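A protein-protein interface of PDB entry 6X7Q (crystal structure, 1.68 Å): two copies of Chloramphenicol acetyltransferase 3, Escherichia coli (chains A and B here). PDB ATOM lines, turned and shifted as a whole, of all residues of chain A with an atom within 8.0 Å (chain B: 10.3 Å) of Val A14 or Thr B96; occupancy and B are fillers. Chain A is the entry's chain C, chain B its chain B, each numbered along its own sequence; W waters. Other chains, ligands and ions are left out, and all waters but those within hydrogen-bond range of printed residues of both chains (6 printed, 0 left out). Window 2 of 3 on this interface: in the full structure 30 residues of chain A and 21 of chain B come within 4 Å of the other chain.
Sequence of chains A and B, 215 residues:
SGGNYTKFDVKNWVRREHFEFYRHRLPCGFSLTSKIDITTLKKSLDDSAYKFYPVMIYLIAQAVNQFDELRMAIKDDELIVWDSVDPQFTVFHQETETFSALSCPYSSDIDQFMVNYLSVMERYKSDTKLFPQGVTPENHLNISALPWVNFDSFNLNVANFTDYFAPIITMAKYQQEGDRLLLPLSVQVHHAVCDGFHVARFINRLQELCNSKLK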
ATOM      1  N   PHE A   8     -31.339  13.287  31.459  1.00  0.00           N
ATOM      2  CA  PHE A   8     -30.083  13.921  31.093  1.00  0.00           C
ATOM      3  C   PHE A   8     -29.859  15.134  31.987  1.00  0.00           C
ATOM      4  O   PHE A   8     -30.800  15.845  32.317  1.00  0.00           O
ATOM      5  CB  PHE A   8     -30.073  14.270  29.602  1.00  0.00           C
ATOM      6  CG  PHE A   8     -28.714  14.604  29.045  1.00  0.00           C
ATOM      7  CD1 PHE A   8     -27.852  13.604  28.626  1.00  0.00           C
ATOM      8  CD2 PHE A   8     -28.286  15.916  28.969  1.00  0.00           C
ATOM      9  CE1 PHE A   8     -26.609  13.904  28.090  1.00  0.00           C
ATOM     10  CE2 PHE A   8     -27.031  16.215  28.458  1.00  0.00           C
ATOM     11  CZ  PHE A   8     -26.196  15.211  28.026  1.00  0.00           C
ATOM     12  N   ASP A   9     -28.616  15.345  32.413  1.00  0.00           N
ATOM     13  CA  ASP A   9     -28.294  16.487  33.255  1.00  0.00           C
ATOM     14  C   ASP A   9     -28.088  17.697  32.344  1.00  0.00           C
ATOM     15  O   ASP A   9     -26.985  17.945  31.871  1.00  0.00           O
ATOM     16  CB  ASP A   9     -27.068  16.140  34.114  1.00  0.00           C
ATOM     17  CG  ASP A   9     -26.550  17.225  35.048  1.00  0.00           C
ATOM     18  OD1 ASP A   9     -27.160  18.313  35.119  1.00  0.00           O
ATOM     19  OD2 ASP A   9     -25.535  16.953  35.709  1.00  0.00           O
ATOM     20  N   VAL A  10     -29.159  18.459  32.121  1.00  0.00           N
ATOM     21  CA  VAL A  10     -29.110  19.615  31.241  1.00  0.00           C
ATOM     22  C   VAL A  10     -28.339  20.749  31.918  1.00  0.00           C
ATOM     23  O   VAL A  10     -27.602  21.489  31.257  1.00  0.00           O
ATOM     24  CB  VAL A  10     -30.529  20.042  30.817  1.00  0.00           C
ATOM     25  CG1 VAL A  10     -30.535  21.390  30.102  1.00  0.00           C
ATOM     26  CG2 VAL A  10     -31.203  18.961  29.975  1.00  0.00           C
ATOM     27  N   LYS A  11     -28.404  20.815  33.256  1.00  0.00           N
ATOM     28  CA  LYS A  11     -27.783  21.928  33.948  1.00  0.00           C
ATOM     29  C   LYS A  11     -26.257  21.870  33.860  1.00  0.00           C
ATOM     30  O   LYS A  11     -25.651  22.929  33.802  1.00  0.00           O
ATOM     31  CB  LYS A  11     -28.341  22.052  35.369  1.00  0.00           C
ATOM     32  CG  LYS A  11     -29.622  22.871  35.373  1.00  0.00           C
ATOM     33  CD  LYS A  11     -30.425  22.896  36.656  1.00  0.00           C
ATOM     34  CE  LYS A  11     -31.751  23.593  36.419  1.00  0.00           C
ATOM     35  NZ  LYS A  11     -32.624  23.591  37.616  1.00  0.00           N
ATOM     36  N   ASN A  12     -25.643  20.680  33.777  1.00  0.00           N
ATOM     37  CA  ASN A  12     -24.197  20.597  33.664  1.00  0.00           C
ATOM     38  C   ASN A  12     -23.770  20.261  32.231  1.00  0.00           C
ATOM     39  O   ASN A  12     -22.603  19.958  31.991  1.00  0.00           O
ATOM     40  CB  ASN A  12     -23.613  19.667  34.731  1.00  0.00           C
ATOM     41  CG  ASN A  12     -23.787  20.227  36.136  1.00  0.00           C
ATOM     42  OD1 ASN A  12     -23.302  21.311  36.468  1.00  0.00           O
ATOM     43  ND2 ASN A  12     -24.548  19.532  36.956  1.00  0.00           N
ATOM     44  N   TRP A  13     -24.701  20.338  31.266  1.00  0.00           N
ATOM     45  CA  TRP A  13     -24.389  20.079  29.865  1.00  0.00           C
ATOM     46  C   TRP A  13     -23.652  21.275  29.265  1.00  0.00           C
ATOM     47  O   TRP A  13     -24.075  22.414  29.418  1.00  0.00           O
ATOM     48  CB  TRP A  13     -25.712  19.860  29.116  1.00  0.00           C
ATOM     49  CG  TRP A  13     -25.650  19.302  27.735  1.00  0.00           C
ATOM     50  CD1 TRP A  13     -24.588  18.712  27.109  1.00  0.00           C
ATOM     51  CD2 TRP A  13     -26.758  19.207  26.829  1.00  0.00           C
ATOM     52  NE1 TRP A  13     -24.961  18.259  25.875  1.00  0.00           N
ATOM     53  CE2 TRP A  13     -26.288  18.542  25.678  1.00  0.00           C
ATOM     54  CE3 TRP A  13     -28.100  19.609  26.890  1.00  0.00           C
ATOM     55  CZ2 TRP A  13     -27.110  18.281  24.582  1.00  0.00           C
ATOM     56  CZ3 TRP A  13     -28.917  19.323  25.815  1.00  0.00           C
ATOM     57  CH2 TRP A  13     -28.417  18.693  24.675  1.00  0.00           C
ATOM     58  N   VAL A  14     -22.637  21.024  28.432  1.00  0.00           N
ATOM     59  CA  VAL A  14     -21.966  22.097  27.714  1.00  0.00           C
ATOM     60  C   VAL A  14     -22.913  22.818  26.736  1.00  0.00           C
ATOM     61  O   VAL A  14     -22.624  23.938  26.345  1.00  0.00           O
ATOM     62  CB  VAL A  14     -20.725  21.548  26.983  1.00  0.00           C
ATOM     63  CG1 VAL A  14     -19.615  21.198  27.980  1.00  0.00           C
ATOM     64  CG2 VAL A  14     -21.036  20.368  26.062  1.00  0.00           C
ATOM     65  N   ARG A  15     -24.019  22.170  26.333  1.00  0.00           N
ATOM     66  CA  ARG A  15     -24.977  22.753  25.398  1.00  0.00           C
ATOM     67  C   ARG A  15     -26.245  23.194  26.120  1.00  0.00           C
ATOM     68  O   ARG A  15     -27.241  23.414  25.455  1.00  0.00           O
ATOM     69  CB  ARG A  15     -25.359  21.754  24.301  1.00  0.00           C
ATOM     70  CG  ARG A  15     -24.222  21.468  23.330  1.00  0.00           C
ATOM     71  CD  ARG A  15     -24.629  20.608  22.164  1.00  0.00           C
ATOM     72  NE  ARG A  15     -25.471  21.342  21.219  1.00  0.00           N
ATOM     73  CZ  ARG A  15     -26.811  21.317  21.193  1.00  0.00           C
ATOM     74  NH1 ARG A  15     -27.505  20.651  22.112  1.00  0.00           N
ATOM     75  NH2 ARG A  15     -27.431  22.026  20.258  1.00  0.00           N
ATOM     76  N   ARG A  16     -26.192  23.364  27.455  1.00  0.00           N
ATOM     77  CA  ARG A  16     -27.344  23.869  28.189  1.00  0.00           C
ATOM     78  C   ARG A  16     -27.985  25.066  27.492  1.00  0.00           C
ATOM     79  O   ARG A  16     -29.209  25.123  27.310  1.00  0.00           O
ATOM     80  CB  ARG A  16     -26.923  24.244  29.620  1.00  0.00           C
ATOM     81  CG  ARG A  16     -28.040  24.844  30.464  1.00  0.00           C
ATOM     82  CD  ARG A  16     -27.538  25.332  31.826  1.00  0.00           C
ATOM     83  NE  ARG A  16     -26.431  26.287  31.751  1.00  0.00           N
ATOM     84  CZ  ARG A  16     -26.484  27.532  31.239  1.00  0.00           C
ATOM     85  NH1 ARG A  16     -27.622  28.072  30.825  1.00  0.00           N
ATOM     86  NH2 ARG A  16     -25.376  28.249  31.131  1.00  0.00           N
ATOM     87  N   GLU A  17     -27.162  26.038  27.101  1.00  0.00           N
ATOM     88  CA  GLU A  17     -27.683  27.267  26.554  1.00  0.00           C
ATOM     89  C   GLU A  17     -28.198  27.084  25.123  1.00  0.00           C
ATOM     90  O   GLU A  17     -29.175  27.724  24.736  1.00  0.00           O
ATOM     91  CB  GLU A  17     -26.603  28.336  26.612  1.00  0.00           C
ATOM     92  CG  GLU A  17     -27.090  29.657  26.094  1.00  0.00           C
ATOM     93  CD  GLU A  17     -26.077  30.761  26.297  1.00  0.00           C
ATOM     94  OE1 GLU A  17     -24.870  30.447  26.500  1.00  0.00           O
ATOM     95  OE2 GLU A  17     -26.496  31.918  26.261  1.00  0.00           O
ATOM     96  N   HIS A  18     -27.542  26.215  24.338  1.00  0.00           N
ATOM     97  CA  HIS A  18     -27.971  25.946  22.961  1.00  0.00           C
ATOM     98  C   HIS A  18     -29.310  25.222  22.951  1.00  0.00           C
ATOM     99  O   HIS A  18     -30.146  25.442  22.054  1.00  0.00           O
ATOM    100  CB  HIS A  18     -26.926  25.109  22.212  1.00  0.00           C
ATOM    101  CG  HIS A  18     -25.560  25.678  22.372  1.00  0.00           C
ATOM    102  ND1 HIS A  18     -24.890  25.703  23.563  1.00  0.00           N
ATOM    103  CD2 HIS A  18     -24.770  26.311  21.458  1.00  0.00           C
ATOM    104  CE1 HIS A  18     -23.723  26.314  23.390  1.00  0.00           C
ATOM    105  NE2 HIS A  18     -23.636  26.718  22.102  1.00  0.00           N
ATOM    106  N   PHE A  19     -29.467  24.272  23.885  1.00  0.00           N
ATOM    107  CA  PHE A  19     -30.682  23.482  24.003  1.00  0.00           C
ATOM    108  C   PHE A  19     -31.862  24.420  24.245  1.00  0.00           C
ATOM    109  O   PHE A  19     -32.861  24.396  23.530  1.00  0.00           O
ATOM    110  CB  PHE A  19     -30.544  22.417  25.094  1.00  0.00           C
ATOM    111  CG  PHE A  19     -31.800  21.620  25.303  1.00  0.00           C
ATOM    112  CD1 PHE A  19     -32.155  20.637  24.396  1.00  0.00           C
ATOM    113  CD2 PHE A  19     -32.615  21.830  26.412  1.00  0.00           C
ATOM    114  CE1 PHE A  19     -33.295  19.862  24.585  1.00  0.00           C
ATOM    115  CE2 PHE A  19     -33.750  21.068  26.590  1.00  0.00           C
ATOM    116  CZ  PHE A  19     -34.085  20.076  25.696  1.00  0.00           C
ATOM    117  N   ASP A 195     -26.035  20.020  16.574  1.00  0.00           N
ATOM    118  CA  ASP A 195     -25.428  21.083  15.769  1.00  0.00           C
ATOM    119  C   ASP A 195     -24.808  20.451  14.496  1.00  0.00           C
ATOM    120  O   ASP A 195     -24.801  19.242  14.313  1.00  0.00           O
ATOM    121  CB  ASP A 195     -24.345  21.806  16.587  1.00  0.00           C
ATOM    122  CG  ASP A 195     -24.800  22.280  17.977  1.00  0.00           C
ATOM    123  OD1 ASP A 195     -25.910  22.786  18.040  1.00  0.00           O
ATOM    124  OD2 ASP A 195     -23.983  22.218  18.957  1.00  0.00           O
ATOM    125  N   PHE A 197     -21.707  20.050  13.876  1.00  0.00           N
ATOM    126  CA  PHE A 197     -20.643  19.161  14.307  1.00  0.00           C
ATOM    127  C   PHE A 197     -21.158  17.731  14.499  1.00  0.00           C
ATOM    128  O   PHE A 197     -20.535  16.779  14.054  1.00  0.00           O
ATOM    129  CB  PHE A 197     -19.968  19.661  15.582  1.00  0.00           C
ATOM    130  CG  PHE A 197     -18.996  18.699  16.211  1.00  0.00           C
ATOM    131  CD1 PHE A 197     -17.694  18.589  15.736  1.00  0.00           C
ATOM    132  CD2 PHE A 197     -19.393  17.890  17.260  1.00  0.00           C
ATOM    133  CE1 PHE A 197     -16.811  17.678  16.302  1.00  0.00           C
ATOM    134  CE2 PHE A 197     -18.511  16.958  17.808  1.00  0.00           C
ATOM    135  CZ  PHE A 197     -17.227  16.885  17.339  1.00  0.00           C
ATOM    136  N   HIS A 198     -22.304  17.560  15.176  1.00  0.00           N
ATOM    137  CA  HIS A 198     -22.786  16.230  15.475  1.00  0.00           C
ATOM    138  C   HIS A 198     -23.295  15.520  14.239  1.00  0.00           C
ATOM    139  O   HIS A 198     -23.162  14.287  14.135  1.00  0.00           O
ATOM    140  CB  HIS A 198     -23.896  16.280  16.558  1.00  0.00           C
ATOM    141  CG  HIS A 198     -23.494  17.091  17.740  1.00  0.00           C
ATOM    142  ND1 HIS A 198     -23.819  18.427  17.850  1.00  0.00           N
ATOM    143  CD2 HIS A 198     -22.657  16.802  18.790  1.00  0.00           C
ATOM    144  CE1 HIS A 198     -23.237  18.931  18.937  1.00  0.00           C
ATOM    145  NE2 HIS A 198     -22.528  17.940  19.545  1.00  0.00           N
ATOM    146  N   VAL B  91     -18.192  30.321  15.740  1.00  0.00           N
ATOM    147  CA  VAL B  91     -16.838  29.889  16.053  1.00  0.00           C
ATOM    148  C   VAL B  91     -16.930  28.608  16.876  1.00  0.00           C
ATOM    149  O   VAL B  91     -17.826  28.444  17.683  1.00  0.00           O
ATOM    150  CB  VAL B  91     -16.035  30.998  16.775  1.00  0.00           C
ATOM    151  CG1 VAL B  91     -16.081  32.284  15.974  1.00  0.00           C
ATOM    152  CG2 VAL B  91     -16.512  31.248  18.186  1.00  0.00           C
ATOM    153  N   PHE B  92     -16.019  27.678  16.630  1.00  0.00           N
ATOM    154  CA  PHE B  92     -16.046  26.382  17.285  1.00  0.00           C
ATOM    155  C   PHE B  92     -15.071  26.358  18.463  1.00  0.00           C
ATOM    156  O   PHE B  92     -14.003  26.965  18.392  1.00  0.00           O
ATOM    157  CB  PHE B  92     -15.669  25.298  16.277  1.00  0.00           C
ATOM    158  CG  PHE B  92     -15.989  23.900  16.723  1.00  0.00           C
ATOM    159  CD1 PHE B  92     -17.311  23.537  16.930  1.00  0.00           C
ATOM    160  CD2 PHE B  92     -14.987  22.966  16.939  1.00  0.00           C
ATOM    161  CE1 PHE B  92     -17.633  22.248  17.309  1.00  0.00           C
ATOM    162  CE2 PHE B  92     -15.308  21.673  17.328  1.00  0.00           C
ATOM    163  CZ  PHE B  92     -16.625  21.332  17.546  1.00  0.00           C
ATOM    164  N   HIS B  93     -15.465  25.652  19.529  1.00  0.00           N
ATOM    165  CA  HIS B  93     -14.614  25.398  20.685  1.00  0.00           C
ATOM    166  C   HIS B  93     -14.285  23.912  20.748  1.00  0.00           C
ATOM    167  O   HIS B  93     -15.115  23.071  21.077  1.00  0.00           O
ATOM    168  CB  HIS B  93     -15.303  25.850  21.966  1.00  0.00           C
ATOM    169  CG  HIS B  93     -15.820  27.250  21.919  1.00  0.00           C
ATOM    170  ND1 HIS B  93     -15.004  28.356  21.815  1.00  0.00           N
ATOM    171  CD2 HIS B  93     -17.101  27.700  22.054  1.00  0.00           C
ATOM    172  CE1 HIS B  93     -15.778  29.443  21.857  1.00  0.00           C
ATOM    173  NE2 HIS B  93     -17.067  29.063  21.982  1.00  0.00           N
ATOM    174  N   GLN B  94     -13.015  23.621  20.450  1.00  0.00           N
ATOM    175  CA  GLN B  94     -12.563  22.258  20.280  1.00  0.00           C
ATOM    176  C   GLN B  94     -12.678  21.513  21.602  1.00  0.00           C
ATOM    177  O   GLN B  94     -12.970  20.331  21.596  1.00  0.00           O
ATOM    178  CB  GLN B  94     -11.123  22.243  19.742  1.00  0.00           C
ATOM    179  CG  GLN B  94     -10.720  20.904  19.149  1.00  0.00           C
ATOM    180  CD  GLN B  94     -11.628  20.505  18.010  1.00  0.00           C
ATOM    181  OE1 GLN B  94     -11.712  21.200  16.994  1.00  0.00           O
ATOM    182  NE2 GLN B  94     -12.343  19.400  18.193  1.00  0.00           N
ATOM    183  N   GLU B  95     -12.460  22.203  22.720  1.00  0.00           N
ATOM    184  CA  GLU B  95     -12.384  21.558  24.023  1.00  0.00           C
ATOM    185  C   GLU B  95     -13.759  21.012  24.431  1.00  0.00           C
ATOM    186  O   GLU B  95     -13.851  19.953  25.055  1.00  0.00           O
ATOM    187  CB  GLU B  95     -11.840  22.547  25.055  1.00  0.00           C
ATOM    188  CG  GLU B  95     -10.657  23.388  24.561  1.00  0.00           C
ATOM    189  CD  GLU B  95     -10.916  24.398  23.434  1.00  0.00           C
ATOM    190  OE1 GLU B  95     -10.014  24.559  22.563  1.00  0.00           O
ATOM    191  OE2 GLU B  95     -12.024  25.011  23.384  1.00  0.00           O
ATOM    192  N   THR B  96     -14.837  21.726  24.073  1.00  0.00           N
ATOM    193  CA  THR B  96     -16.188  21.369  24.491  1.00  0.00           C
ATOM    194  C   THR B  96     -17.053  20.820  23.343  1.00  0.00           C
ATOM    195  O   THR B  96     -18.136  20.318  23.617  1.00  0.00           O
ATOM    196  CB  THR B  96     -16.930  22.564  25.105  1.00  0.00           C
ATOM    197  OG1 THR B  96     -16.824  23.631  24.174  1.00  0.00           O
ATOM    198  CG2 THR B  96     -16.388  23.005  26.452  1.00  0.00           C
ATOM    199  N   GLU B  97     -16.596  20.956  22.091  1.00  0.00           N
ATOM    200  CA  GLU B  97     -17.332  20.580  20.885  1.00  0.00           C
ATOM    201  C   GLU B  97     -18.665  21.339  20.818  1.00  0.00           C
ATOM    202  O   GLU B  97     -19.676  20.791  20.360  1.00  0.00           O
ATOM    203  CB  GLU B  97     -17.450  19.056  20.761  1.00  0.00           C
ATOM    204  CG  GLU B  97     -16.087  18.383  20.517  1.00  0.00           C
ATOM    205  CD  GLU B  97     -16.046  16.855  20.550  1.00  0.00           C
ATOM    206  OE1 GLU B  97     -16.997  16.240  21.043  1.00  0.00           O
ATOM    207  OE2 GLU B  97     -15.058  16.292  20.034  1.00  0.00           O
ATOM    208  N   THR B  98     -18.613  22.634  21.190  1.00  0.00           N
ATOM    209  CA  THR B  98     -19.740  23.557  21.118  1.00  0.00           C
ATOM    210  C   THR B  98     -19.306  24.783  20.319  1.00  0.00           C
ATOM    211  O   THR B  98     -18.117  25.006  20.064  1.00  0.00           O
ATOM    212  CB  THR B  98     -20.305  23.910  22.506  1.00  0.00           C
ATOM    213  OG1 THR B  98     -19.297  24.640  23.218  1.00  0.00           O
ATOM    214  CG2 THR B  98     -20.753  22.687  23.291  1.00  0.00           C
ATOM    215  N   PHE B  99     -20.288  25.575  19.903  1.00  0.00           N
ATOM    216  CA  PHE B  99     -20.012  26.788  19.159  1.00  0.00           C
ATOM    217  C   PHE B  99     -20.608  27.994  19.876  1.00  0.00           C
ATOM    218  O   PHE B  99     -21.462  27.906  20.766  1.00  0.00           O
ATOM    219  CB  PHE B  99     -20.548  26.718  17.718  1.00  0.00           C
ATOM    220  CG  PHE B  99     -22.056  26.808  17.591  1.00  0.00           C
ATOM    221  CD1 PHE B  99     -22.854  25.676  17.709  1.00  0.00           C
ATOM    222  CD2 PHE B  99     -22.671  28.026  17.340  1.00  0.00           C
ATOM    223  CE1 PHE B  99     -24.243  25.756  17.586  1.00  0.00           C
ATOM    224  CE2 PHE B  99     -24.052  28.116  17.239  1.00  0.00           C
ATOM    225  CZ  PHE B  99     -24.836  26.985  17.361  1.00  0.00           C
ATOM    226  N   SER B 100     -20.139  29.147  19.436  1.00  0.00           N
ATOM    227  CA  SER B 100     -20.671  30.444  19.827  1.00  0.00           C
ATOM    228  C   SER B 100     -20.899  31.276  18.559  1.00  0.00           C
ATOM    229  O   SER B 100     -20.258  31.054  17.547  1.00  0.00           O
ATOM    230  CB  SER B 100     -19.733  31.208  20.746  1.00  0.00           C
ATOM    231  OG  SER B 100     -19.435  30.477  21.925  1.00  0.00           O
ATOM    232  N   LYS B 125     -12.963  34.545  21.917  1.00  0.00           N
ATOM    233  CA  LYS B 125     -12.919  33.265  21.222  1.00  0.00           C
ATOM    234  C   LYS B 125     -13.016  32.094  22.205  1.00  0.00           C
ATOM    235  O   LYS B 125     -13.417  31.004  21.794  1.00  0.00           O
ATOM    236  CB  LYS B 125     -11.628  33.089  20.419  1.00  0.00           C
ATOM    237  CG  LYS B 125     -10.368  33.154  21.284  1.00  0.00           C
ATOM    238  CD  LYS B 125      -9.156  32.501  20.681  1.00  0.00           C
ATOM    239  CE  LYS B 125      -8.730  33.163  19.400  1.00  0.00           C
ATOM    240  NZ  LYS B 125      -7.623  32.398  18.801  1.00  0.00           N
ATOM    241  N   SER B 126     -12.615  32.277  23.471  1.00  0.00           N
ATOM    242  CA  SER B 126     -12.621  31.149  24.403  1.00  0.00           C
ATOM    243  C   SER B 126     -13.879  31.101  25.289  1.00  0.00           C
ATOM    244  O   SER B 126     -14.033  30.198  26.111  1.00  0.00           O
ATOM    245  CB  SER B 126     -11.378  31.184  25.239  1.00  0.00           C
ATOM    246  OG  SER B 126     -10.282  30.698  24.470  1.00  0.00           O
ATOM    247  N   ASP B 127     -14.788  32.067  25.125  1.00  0.00           N
ATOM    248  CA  ASP B 127     -16.022  32.151  25.887  1.00  0.00           C
ATOM    249  C   ASP B 127     -17.031  31.177  25.273  1.00  0.00           C
ATOM    250  O   ASP B 127     -17.429  31.364  24.124  1.00  0.00           O
ATOM    251  CB  ASP B 127     -16.549  33.589  25.877  1.00  0.00           C
ATOM    252  CG  ASP B 127     -17.757  33.876  26.760  1.00  0.00           C
ATOM    253  OD1 ASP B 127     -18.357  32.926  27.257  1.00  0.00           O
ATOM    254  OD2 ASP B 127     -18.018  35.077  27.010  1.00  0.00           O
ATOM    255  N   THR B 128     -17.505  30.224  26.070  1.00  0.00           N
ATOM    256  CA  THR B 128     -18.411  29.190  25.583  1.00  0.00           C
ATOM    257  C   THR B 128     -19.875  29.654  25.647  1.00  0.00           C
ATOM    258  O   THR B 128     -20.744  28.883  25.260  1.00  0.00           O
ATOM    259  CB  THR B 128     -18.233  27.853  26.321  1.00  0.00           C
ATOM    260  OG1 THR B 128     -18.434  28.140  27.710  1.00  0.00           O
ATOM    261  CG2 THR B 128     -16.875  27.208  26.126  1.00  0.00           C
ATOM    262  N   LYS B 129     -20.169  30.887  26.110  1.00  0.00           N
ATOM    263  CA  LYS B 129     -21.529  31.405  26.001  1.00  0.00           C
ATOM    264  C   LYS B 129     -21.941  31.417  24.532  1.00  0.00           C
ATOM    265  O   LYS B 129     -21.097  31.559  23.654  1.00  0.00           O
ATOM    266  CB  LYS B 129     -21.662  32.800  26.626  1.00  0.00           C
ATOM    267  CG  LYS B 129     -21.779  32.783  28.146  1.00  0.00           C
ATOM    268  CD  LYS B 129     -22.107  34.135  28.759  1.00  0.00           C
ATOM    269  CE  LYS B 129     -20.990  35.155  28.648  1.00  0.00           C
ATOM    270  NZ  LYS B 129     -19.791  34.768  29.433  1.00  0.00           N
ATOM    271  N   LEU B 130     -23.237  31.207  24.261  1.00  0.00           N
ATOM    272  CA  LEU B 130     -23.725  31.205  22.893  1.00  0.00           C
ATOM    273  C   LEU B 130     -23.519  32.585  22.270  1.00  0.00           C
ATOM    274  O   LEU B 130     -23.063  32.672  21.124  1.00  0.00           O
ATOM    275  CB  LEU B 130     -25.197  30.778  22.831  1.00  0.00           C
ATOM    276  CG  LEU B 130     -25.845  30.890  21.453  1.00  0.00           C
ATOM    277  CD1 LEU B 130     -25.083  30.037  20.445  1.00  0.00           C
ATOM    278  CD2 LEU B 130     -27.304  30.474  21.507  1.00  0.00           C
ATOM    279  N   TRP B 148     -16.553  20.105   8.560  1.00  0.00           N
ATOM    280  CA  TRP B 148     -16.229  18.707   8.798  1.00  0.00           C
ATOM    281  C   TRP B 148     -16.875  17.751   7.798  1.00  0.00           C
ATOM    282  O   TRP B 148     -16.495  16.581   7.792  1.00  0.00           O
ATOM    283  CB  TRP B 148     -16.650  18.281  10.198  1.00  0.00           C
ATOM    284  CG  TRP B 148     -16.286  19.270  11.260  1.00  0.00           C
ATOM    285  CD1 TRP B 148     -15.073  19.437  11.879  1.00  0.00           C
ATOM    286  CD2 TRP B 148     -17.164  20.277  11.777  1.00  0.00           C
ATOM    287  NE1 TRP B 148     -15.148  20.470  12.792  1.00  0.00           N
ATOM    288  CE2 TRP B 148     -16.433  20.977  12.767  1.00  0.00           C
ATOM    289  CE3 TRP B 148     -18.517  20.592  11.567  1.00  0.00           C
ATOM    290  CZ2 TRP B 148     -17.020  21.991  13.514  1.00  0.00           C
ATOM    291  CZ3 TRP B 148     -19.078  21.615  12.296  1.00  0.00           C
ATOM    292  CH2 TRP B 148     -18.341  22.285  13.261  1.00  0.00           C
HETATM  293  O   HOH W   1     -20.907  18.593  21.675  1.00  0.00           O
HETATM  294  O   HOH W   2     -22.842  24.020  20.658  1.00  0.00           O
HETATM  295  O   HOH W   3     -21.294  21.993  18.234  1.00  0.00           O
HETATM  296  O   HOH W   4     -20.334  27.167  23.160  1.00  0.00           O
HETATM  297  O   HOH W   5     -20.143  24.927  26.480  1.00  0.00           O
HETATM  298  O   HOH W   6     -23.166  28.291  26.648  1.00  0.00           O
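O of Phe B99 lies within hydrogen-bond range of NE2 of His A18 (2.8 Å). N of Leu B130 is in hydrogen-bond range of OE1 of Glu A17, at 2.9 Å.
The backbone NH (N) of His B93 lies within hydrogen-bond range of the backbone carbonyl oxygen (O) of Thr B98 (2.8 Å). OG1 of Thr B98 sits at hydrogen-bond distance from OG1 of Thr B96 (2.8 Å). The side-chain hydroxyl (OG) of Ser B100 is in hydrogen-bond range of the backbone carbonyl oxygen (O) of Lys B129 (2.6 Å). OD2 of Asp B127 is in salt-bridge range of NZ of Lys B129, 3.0 Å away. The side-chain carboxylate (OD1) of Asp A195 is in salt-bridge range of the guanidinium group (NH2) of Arg A15, 2.8 Å away. The backbone NH of Asp A195 is in hydrogen-bond range of a ring nitrogen (ND1) of His A198, 3.0 Å away.
O of Thr B96 touches CG2 of Val A14 (3.8 Å). Thr B98 touches Val A14. CG of Arg A15 touches CG2 of Thr B98, at 3.7 Å. Lys B129 touches Glu A17. Leu B130 touches His A18 (CD1 to CD2, 3.9 Å). Asp A195 touches Phe B99 (OD1 to CE1, 3.4 Å). CD1 of Phe A197 touches CZ of Phe B92, at 3.5 Å. Phe A197 touches Glu B97. Phe A197 touches Trp B148.
Of the printed residues of chain B, Glu A17 touches Lys B129 (3.5 Å) and Leu B130 (2.9 Å). Printed residues of chain A within 4 Å of Phe B92: Phe A197. Glu B95 touches none of the printed residues of chain A. Thr B96 touches one residue of chain A. Printed residues of chain A within 4 Å of Thr B98: Val A14 (3.6 Å) and Arg A15 (3.7 Å). Thr B128 touches none of the printed residues of chain A. The nearest residue of chain B that does not touch Val A14 is Thr B128 (5.4 Å). The nearest residue of chain A that does not touch Thr B96 is Arg A15 (6.2 Å).
Of the 15 printed residues of chain A, 6 touch a printed residue of chain B. Printed residues of chain A that touch a printed residue of chain B: Val A14, Arg A15, Glu A17, His A18, Asp A195 and Phe A197. Among the printed residues, 11 pairs touch across the chains. Among the printed residues, no Asp or Glu carboxylate lies within 4 Å of a Lys or Arg side-chain nitrogen of the other chain.
No position is printed for both chains. Of the 11 pairs that touch across the chains among the printed residues, none has its exchanged pair printed and touching as well.
Water W5 lies within hydrogen-bond range of O of Val A14 (2.7 Å) and OG1 of Thr B98 (3.4 Å). Water W2 lies within hydrogen-bond range of OD2 of Asp A195, N of Phe B99 and NE2 of His A18. Water W4 lies within hydrogen-bond range of the side-chain hydroxyl (OG1) of Thr B98 (2.7 Å), the backbone carbonyl oxygen (O) of Thr B128 (2.7 Å), the backbone carbonyl oxygen (O) of Phe B99 (2.7 Å) and a ring nitrogen (NE2) of His A18 (3.5 Å). Water W6 bridges OE1 of Glu A17 (2.8 Å) and O of Thr B128 (2.9 Å). Water W1 lies within hydrogen-bond range of NE2 of His A198 and O of Glu B97. Water W3 bridges OD2 of Asp A195 (2.8 Å) and O of Glu B97 (2.9 Å).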
